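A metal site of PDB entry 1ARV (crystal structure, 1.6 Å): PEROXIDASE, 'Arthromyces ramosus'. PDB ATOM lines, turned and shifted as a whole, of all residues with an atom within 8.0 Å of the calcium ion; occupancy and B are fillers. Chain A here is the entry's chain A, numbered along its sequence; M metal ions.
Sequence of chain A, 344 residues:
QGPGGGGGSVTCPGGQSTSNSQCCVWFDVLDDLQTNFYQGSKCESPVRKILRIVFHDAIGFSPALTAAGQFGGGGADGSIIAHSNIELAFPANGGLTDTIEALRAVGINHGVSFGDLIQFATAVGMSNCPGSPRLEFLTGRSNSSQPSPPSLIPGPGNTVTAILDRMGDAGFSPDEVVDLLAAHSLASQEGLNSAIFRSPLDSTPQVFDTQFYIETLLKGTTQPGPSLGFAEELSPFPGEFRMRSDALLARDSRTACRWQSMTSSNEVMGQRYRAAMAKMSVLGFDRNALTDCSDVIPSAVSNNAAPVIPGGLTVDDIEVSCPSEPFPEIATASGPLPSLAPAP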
ATOM      1  N   PRO A 130      -8.399  17.080 -26.101  1.00  0.00           N
ATOM      2  CA  PRO A 130      -9.297  16.239 -25.295  1.00  0.00           C
ATOM      3  C   PRO A 130      -8.560  15.122 -24.581  1.00  0.00           C
ATOM      4  O   PRO A 130      -7.683  14.484 -25.152  1.00  0.00           O
ATOM      5  CB  PRO A 130     -10.306  15.683 -26.277  1.00  0.00           C
ATOM      6  CG  PRO A 130     -10.299  16.675 -27.412  1.00  0.00           C
ATOM      7  CD  PRO A 130      -8.867  17.166 -27.477  1.00  0.00           C
ATOM      8  N   ALA A 182       4.084   9.377 -23.222  1.00  0.00           N
ATOM      9  CA  ALA A 182       2.647   9.511 -23.474  1.00  0.00           C
ATOM     10  C   ALA A 182       2.450  10.704 -24.422  1.00  0.00           C
ATOM     11  O   ALA A 182       1.452  10.771 -25.124  1.00  0.00           O
ATOM     12  CB  ALA A 182       1.840   9.794 -22.178  1.00  0.00           C
ATOM     13  N   ALA A 183       3.376  11.681 -24.485  1.00  0.00           N
ATOM     14  CA  ALA A 183       3.236  12.794 -25.402  1.00  0.00           C
ATOM     15  C   ALA A 183       3.245  12.328 -26.867  1.00  0.00           C
ATOM     16  O   ALA A 183       2.738  13.033 -27.730  1.00  0.00           O
ATOM     17  CB  ALA A 183       4.371  13.759 -25.221  1.00  0.00           C
ATOM     18  N   HIS A 184       3.720  11.112 -27.203  1.00  0.00           N
ATOM     19  CA  HIS A 184       3.631  10.650 -28.569  1.00  0.00           C
ATOM     20  C   HIS A 184       2.191  10.211 -28.931  1.00  0.00           C
ATOM     21  O   HIS A 184       1.892   9.767 -30.056  1.00  0.00           O
ATOM     22  CB  HIS A 184       4.633   9.518 -28.805  1.00  0.00           C
ATOM     23  CG  HIS A 184       6.061   9.980 -29.089  1.00  0.00           C
ATOM     24  ND1 HIS A 184       7.040   9.142 -29.606  1.00  0.00           N
ATOM     25  CD2 HIS A 184       6.599  11.264 -28.921  1.00  0.00           C
ATOM     26  CE1 HIS A 184       8.136   9.894 -29.798  1.00  0.00           C
ATOM     27  NE2 HIS A 184       7.908  11.109 -29.407  1.00  0.00           N
ATOM     28  N   SER A 185       1.234  10.357 -27.986  1.00  0.00           N
ATOM     29  CA  SER A 185      -0.177  10.138 -28.269  1.00  0.00           C
ATOM     30  C   SER A 185      -0.700  11.394 -28.980  1.00  0.00           C
ATOM     31  O   SER A 185      -1.816  11.361 -29.515  1.00  0.00           O
ATOM     32  CB  SER A 185      -0.967   9.929 -26.971  1.00  0.00           C
ATOM     33  OG  SER A 185      -2.332   9.577 -27.201  1.00  0.00           O
ATOM     34  N   LEU A 186       0.039  12.522 -29.046  1.00  0.00           N
ATOM     35  CA  LEU A 186      -0.390  13.746 -29.711  1.00  0.00           C
ATOM     36  C   LEU A 186       0.756  14.046 -30.675  1.00  0.00           C
ATOM     37  O   LEU A 186       1.419  15.100 -30.587  1.00  0.00           O
ATOM     38  CB  LEU A 186      -0.542  14.789 -28.625  1.00  0.00           C
ATOM     39  CG  LEU A 186      -1.828  15.290 -27.974  1.00  0.00           C
ATOM     40  CD1 LEU A 186      -2.981  14.369 -28.136  1.00  0.00           C
ATOM     41  CD2 LEU A 186      -1.467  15.571 -26.531  1.00  0.00           C
ATOM     42  N   ALA A 187       1.005  13.176 -31.660  1.00  0.00           N
ATOM     43  CA  ALA A 187       2.215  13.317 -32.473  1.00  0.00           C
ATOM     44  C   ALA A 187       2.152  12.849 -33.900  1.00  0.00           C
ATOM     45  O   ALA A 187       1.343  11.990 -34.283  1.00  0.00           O
ATOM     46  CB  ALA A 187       3.347  12.559 -31.780  1.00  0.00           C
ATOM     47  N   LEU A 201       1.593   9.250 -35.132  1.00  0.00           N
ATOM     48  CA  LEU A 201       2.237   8.166 -34.415  1.00  0.00           C
ATOM     49  C   LEU A 201       1.149   7.276 -33.786  1.00  0.00           C
ATOM     50  O   LEU A 201       1.432   6.154 -33.359  1.00  0.00           O
ATOM     51  CB  LEU A 201       3.186   8.768 -33.409  1.00  0.00           C
ATOM     52  CG  LEU A 201       4.692   8.785 -33.771  1.00  0.00           C
ATOM     53  CD1 LEU A 201       4.952   9.122 -35.228  1.00  0.00           C
ATOM     54  CD2 LEU A 201       5.382   9.716 -32.797  1.00  0.00           C
ATOM     55  N   ASP A 202      -0.101   7.738 -33.628  1.00  0.00           N
ATOM     56  CA  ASP A 202      -1.154   6.823 -33.207  1.00  0.00           C
ATOM     57  C   ASP A 202      -2.399   7.239 -33.970  1.00  0.00           C
ATOM     58  O   ASP A 202      -2.368   8.249 -34.694  1.00  0.00           O
ATOM     59  CB  ASP A 202      -1.419   6.834 -31.669  1.00  0.00           C
ATOM     60  CG  ASP A 202      -2.174   7.956 -30.937  1.00  0.00           C
ATOM     61  OD1 ASP A 202      -2.641   8.939 -31.547  1.00  0.00           O
ATOM     62  OD2 ASP A 202      -2.272   7.835 -29.716  1.00  0.00           O
ATOM     63  N   SER A 203      -3.519   6.526 -33.820  1.00  0.00           N
ATOM     64  CA  SER A 203      -4.714   6.843 -34.585  1.00  0.00           C
ATOM     65  C   SER A 203      -5.509   8.023 -34.083  1.00  0.00           C
ATOM     66  O   SER A 203      -6.537   8.356 -34.682  1.00  0.00           O
ATOM     67  CB  SER A 203      -5.616   5.596 -34.637  1.00  0.00           C
ATOM     68  OG  SER A 203      -5.994   5.146 -33.347  1.00  0.00           O
ATOM     69  N   THR A 204      -5.158   8.659 -32.964  1.00  0.00           N
ATOM     70  CA  THR A 204      -5.881   9.813 -32.491  1.00  0.00           C
ATOM     71  C   THR A 204      -4.851  10.893 -32.194  1.00  0.00           C
ATOM     72  O   THR A 204      -4.609  11.172 -31.011  1.00  0.00           O
ATOM     73  CB  THR A 204      -6.654   9.391 -31.248  1.00  0.00           C
ATOM     74  OG1 THR A 204      -5.699   8.760 -30.407  1.00  0.00           O
ATOM     75  CG2 THR A 204      -7.805   8.435 -31.515  1.00  0.00           C
ATOM     76  N   PRO A 205      -4.192  11.563 -33.169  1.00  0.00           N
ATOM     77  CA  PRO A 205      -3.184  12.610 -32.883  1.00  0.00           C
ATOM     78  C   PRO A 205      -3.744  13.846 -32.180  1.00  0.00           C
ATOM     79  O   PRO A 205      -2.982  14.757 -31.799  1.00  0.00           O
ATOM     80  CB  PRO A 205      -2.580  12.923 -34.260  1.00  0.00           C
ATOM     81  CG  PRO A 205      -3.720  12.605 -35.228  1.00  0.00           C
ATOM     82  CD  PRO A 205      -4.329  11.346 -34.607  1.00  0.00           C
ATOM     83  N   GLN A 206      -5.075  13.925 -32.055  1.00  0.00           N
ATOM     84  CA  GLN A 206      -5.692  15.047 -31.385  1.00  0.00           C
ATOM     85  C   GLN A 206      -6.377  14.617 -30.094  1.00  0.00           C
ATOM     86  O   GLN A 206      -7.204  15.363 -29.575  1.00  0.00           O
ATOM     87  CB  GLN A 206      -6.697  15.718 -32.329  1.00  0.00           C
ATOM     88  CG  GLN A 206      -6.045  16.460 -33.490  1.00  0.00           C
ATOM     89  CD  GLN A 206      -7.074  17.277 -34.271  1.00  0.00           C
ATOM     90  OE1 GLN A 206      -7.897  16.709 -34.989  1.00  0.00           O
ATOM     91  NE2 GLN A 206      -7.051  18.597 -34.199  1.00  0.00           N
ATOM     92  N   VAL A 207      -6.119  13.429 -29.551  1.00  0.00           N
ATOM     93  CA  VAL A 207      -6.739  12.984 -28.305  1.00  0.00           C
ATOM     94  C   VAL A 207      -5.604  12.425 -27.438  1.00  0.00           C
ATOM     95  O   VAL A 207      -4.809  11.594 -27.922  1.00  0.00           O
ATOM     96  CB  VAL A 207      -7.796  11.869 -28.527  1.00  0.00           C
ATOM     97  CG1 VAL A 207      -8.392  11.500 -27.185  1.00  0.00           C
ATOM     98  CG2 VAL A 207      -8.920  12.339 -29.411  1.00  0.00           C
ATOM     99  N   PHE A 208      -5.480  12.865 -26.181  1.00  0.00           N
ATOM    100  CA  PHE A 208      -4.419  12.405 -25.293  1.00  0.00           C
ATOM    101  C   PHE A 208      -4.988  11.163 -24.640  1.00  0.00           C
ATOM    102  O   PHE A 208      -5.793  11.231 -23.698  1.00  0.00           O
ATOM    103  CB  PHE A 208      -4.115  13.466 -24.239  1.00  0.00           C
ATOM    104  CG  PHE A 208      -2.974  13.081 -23.324  1.00  0.00           C
ATOM    105  CD1 PHE A 208      -1.678  13.059 -23.814  1.00  0.00           C
ATOM    106  CD2 PHE A 208      -3.238  12.772 -22.007  1.00  0.00           C
ATOM    107  CE1 PHE A 208      -0.639  12.719 -22.970  1.00  0.00           C
ATOM    108  CE2 PHE A 208      -2.208  12.432 -21.183  1.00  0.00           C
ATOM    109  CZ  PHE A 208      -0.909  12.406 -21.664  1.00  0.00           C
ATOM    110  N   ASP A 209      -4.594  10.034 -25.211  1.00  0.00           N
ATOM    111  CA  ASP A 209      -5.105   8.755 -24.782  1.00  0.00           C
ATOM    112  C   ASP A 209      -4.032   7.662 -24.852  1.00  0.00           C
ATOM    113  O   ASP A 209      -2.876   7.814 -25.252  1.00  0.00           O
ATOM    114  CB  ASP A 209      -6.332   8.435 -25.672  1.00  0.00           C
ATOM    115  CG  ASP A 209      -6.020   8.319 -27.165  1.00  0.00           C
ATOM    116  OD1 ASP A 209      -4.856   8.302 -27.581  1.00  0.00           O
ATOM    117  OD2 ASP A 209      -6.952   8.228 -27.957  1.00  0.00           O
ATOM    118  N   THR A 210      -4.460   6.489 -24.525  1.00  0.00           N
ATOM    119  CA  THR A 210      -3.681   5.286 -24.491  1.00  0.00           C
ATOM    120  C   THR A 210      -3.330   4.634 -25.847  1.00  0.00           C
ATOM    121  O   THR A 210      -2.468   3.732 -25.937  1.00  0.00           O
ATOM    122  CB  THR A 210      -4.608   4.586 -23.509  1.00  0.00           C
ATOM    123  OG1 THR A 210      -3.962   4.555 -22.250  1.00  0.00           O
ATOM    124  CG2 THR A 210      -5.181   3.398 -24.129  1.00  0.00           C
ATOM    125  N   GLN A 211      -3.974   5.059 -26.954  1.00  0.00           N
ATOM    126  CA  GLN A 211      -3.786   4.433 -28.260  1.00  0.00           C
ATOM    127  C   GLN A 211      -2.352   4.292 -28.698  1.00  0.00           C
ATOM    128  O   GLN A 211      -2.023   3.259 -29.275  1.00  0.00           O
ATOM    129  CB  GLN A 211      -4.540   5.189 -29.343  1.00  0.00           C
ATOM    130  CG  GLN A 211      -6.052   5.103 -29.188  1.00  0.00           C
ATOM    131  CD  GLN A 211      -6.625   3.679 -29.061  1.00  0.00           C
ATOM    132  OE1 GLN A 211      -7.436   3.420 -28.158  1.00  0.00           O
ATOM    133  NE2 GLN A 211      -6.280   2.722 -29.902  1.00  0.00           N
ATOM    134  N   PHE A 212      -1.479   5.247 -28.429  1.00  0.00           N
ATOM    135  CA  PHE A 212      -0.066   5.115 -28.794  1.00  0.00           C
ATOM    136  C   PHE A 212       0.562   3.886 -28.154  1.00  0.00           C
ATOM    137  O   PHE A 212       1.301   3.184 -28.857  1.00  0.00           O
ATOM    138  CB  PHE A 212       0.688   6.392 -28.370  1.00  0.00           C
ATOM    139  CG  PHE A 212       2.205   6.250 -28.380  1.00  0.00           C
ATOM    140  CD1 PHE A 212       2.885   6.217 -29.584  1.00  0.00           C
ATOM    141  CD2 PHE A 212       2.867   6.133 -27.176  1.00  0.00           C
ATOM    142  CE1 PHE A 212       4.257   6.072 -29.568  1.00  0.00           C
ATOM    143  CE2 PHE A 212       4.233   5.984 -27.172  1.00  0.00           C
ATOM    144  CZ  PHE A 212       4.919   5.955 -28.364  1.00  0.00           C
ATOM    145  N   TYR A 213       0.301   3.557 -26.897  1.00  0.00           N
ATOM    146  CA  TYR A 213       0.915   2.393 -26.287  1.00  0.00           C
ATOM    147  C   TYR A 213       0.392   1.107 -26.908  1.00  0.00           C
ATOM    148  O   TYR A 213       1.157   0.169 -27.176  1.00  0.00           O
ATOM    149  CB  TYR A 213       0.642   2.471 -24.793  1.00  0.00           C
ATOM    150  CG  TYR A 213       1.375   3.654 -24.113  1.00  0.00           C
ATOM    151  CD1 TYR A 213       2.750   3.609 -23.908  1.00  0.00           C
ATOM    152  CD2 TYR A 213       0.672   4.760 -23.675  1.00  0.00           C
ATOM    153  CE1 TYR A 213       3.422   4.643 -23.256  1.00  0.00           C
ATOM    154  CE2 TYR A 213       1.335   5.794 -23.019  1.00  0.00           C
ATOM    155  CZ  TYR A 213       2.698   5.729 -22.809  1.00  0.00           C
ATOM    156  OH  TYR A 213       3.322   6.735 -22.107  1.00  0.00           O
ATOM    157  N   GLU A 215      -1.022   0.667 -30.044  1.00  0.00           N
ATOM    158  CA  GLU A 215      -0.634   0.565 -31.448  1.00  0.00           C
ATOM    159  C   GLU A 215       0.837   0.323 -31.716  1.00  0.00           C
ATOM    160  O   GLU A 215       1.108  -0.333 -32.708  1.00  0.00           O
ATOM    161  CB  GLU A 215      -1.151   1.824 -32.147  1.00  0.00           C
ATOM    162  CG  GLU A 215      -2.698   1.794 -32.140  1.00  0.00           C
ATOM    163  CD  GLU A 215      -3.377   3.043 -32.654  1.00  0.00           C
ATOM    164  OE1 GLU A 215      -2.756   3.845 -33.347  1.00  0.00           O
ATOM    165  OE2 GLU A 215      -4.532   3.237 -32.334  1.00  0.00           O
ATOM    166  N   ASN A 266      -6.708   5.493 -19.401  1.00  0.00           N
ATOM    167  CA  ASN A 266      -6.378   6.864 -19.700  1.00  0.00           C
ATOM    168  C   ASN A 266      -6.138   7.639 -18.413  1.00  0.00           C
ATOM    169  O   ASN A 266      -5.303   8.539 -18.354  1.00  0.00           O
ATOM    170  CB  ASN A 266      -7.503   7.538 -20.443  1.00  0.00           C
ATOM    171  CG  ASN A 266      -7.629   7.106 -21.900  1.00  0.00           C
ATOM    172  OD1 ASN A 266      -6.643   7.017 -22.631  1.00  0.00           O
ATOM    173  ND2 ASN A 266      -8.825   6.834 -22.399  1.00  0.00           N
ATOM    174  N   MET A 269      -2.550   6.744 -17.111  1.00  0.00           N
ATOM    175  CA  MET A 269      -1.564   7.333 -17.997  1.00  0.00           C
ATOM    176  C   MET A 269      -1.479   8.822 -17.730  1.00  0.00           C
ATOM    177  O   MET A 269      -0.391   9.366 -17.520  1.00  0.00           O
ATOM    178  CB  MET A 269      -1.957   7.093 -19.453  1.00  0.00           C
ATOM    179  CG  MET A 269      -1.062   7.849 -20.404  1.00  0.00           C
ATOM    180  SD  MET A 269      -1.689   7.746 -22.108  1.00  0.00           S
ATOM    181  CE  MET A 269      -2.808   9.102 -21.969  1.00  0.00           C
ATOM    182  N   ASN A 303     -12.213  13.033 -22.451  1.00  0.00           N
ATOM    183  CA  ASN A 303     -12.205  12.067 -23.513  1.00  0.00           C
ATOM    184  C   ASN A 303     -13.104  10.950 -22.997  1.00  0.00           C
ATOM    185  O   ASN A 303     -12.836  10.323 -21.980  1.00  0.00           O
ATOM    186  CB  ASN A 303     -10.811  11.526 -23.743  1.00  0.00           C
ATOM    187  CG  ASN A 303     -10.822  10.293 -24.627  1.00  0.00           C
ATOM    188  OD1 ASN A 303     -11.717  10.122 -25.453  1.00  0.00           O
ATOM    189  ND2 ASN A 303      -9.871   9.388 -24.496  1.00  0.00           N
HETATM  190 CA    CA M   1      -3.695   9.751 -29.256  1.00  0.00          CA
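The side-chain carboxylate (OD1) of Asp 209 lies close to the backbone NH (N) of Gln 211, 3.4 Å away. OD2 of Asp 202 sits close to N of Phe 212, 3.0 Å away.
Of the 24 residues printed, 5 come within 4 Å of the calcium ion.
The calcium ion is bound by the side-chain carboxylate (OD2) of Asp 202 (2.4 Å), the backbone carbonyl oxygen (O) of Thr 204 (2.4 Å), the side-chain hydroxyl (OG) of Ser 185 (2.5 Å), the backbone carbonyl oxygen (O) of Ser 185 (2.5 Å), the side-chain carboxylate (OD1) of Asp 209 (2.5 Å), the side-chain hydroxyl (OG1) of Thr 204 (2.5 Å), the backbone carbonyl oxygen (O) of Val 207 (2.5 Å) and the side-chain carboxylate (OD1) of Asp 202 (2.6 Å).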
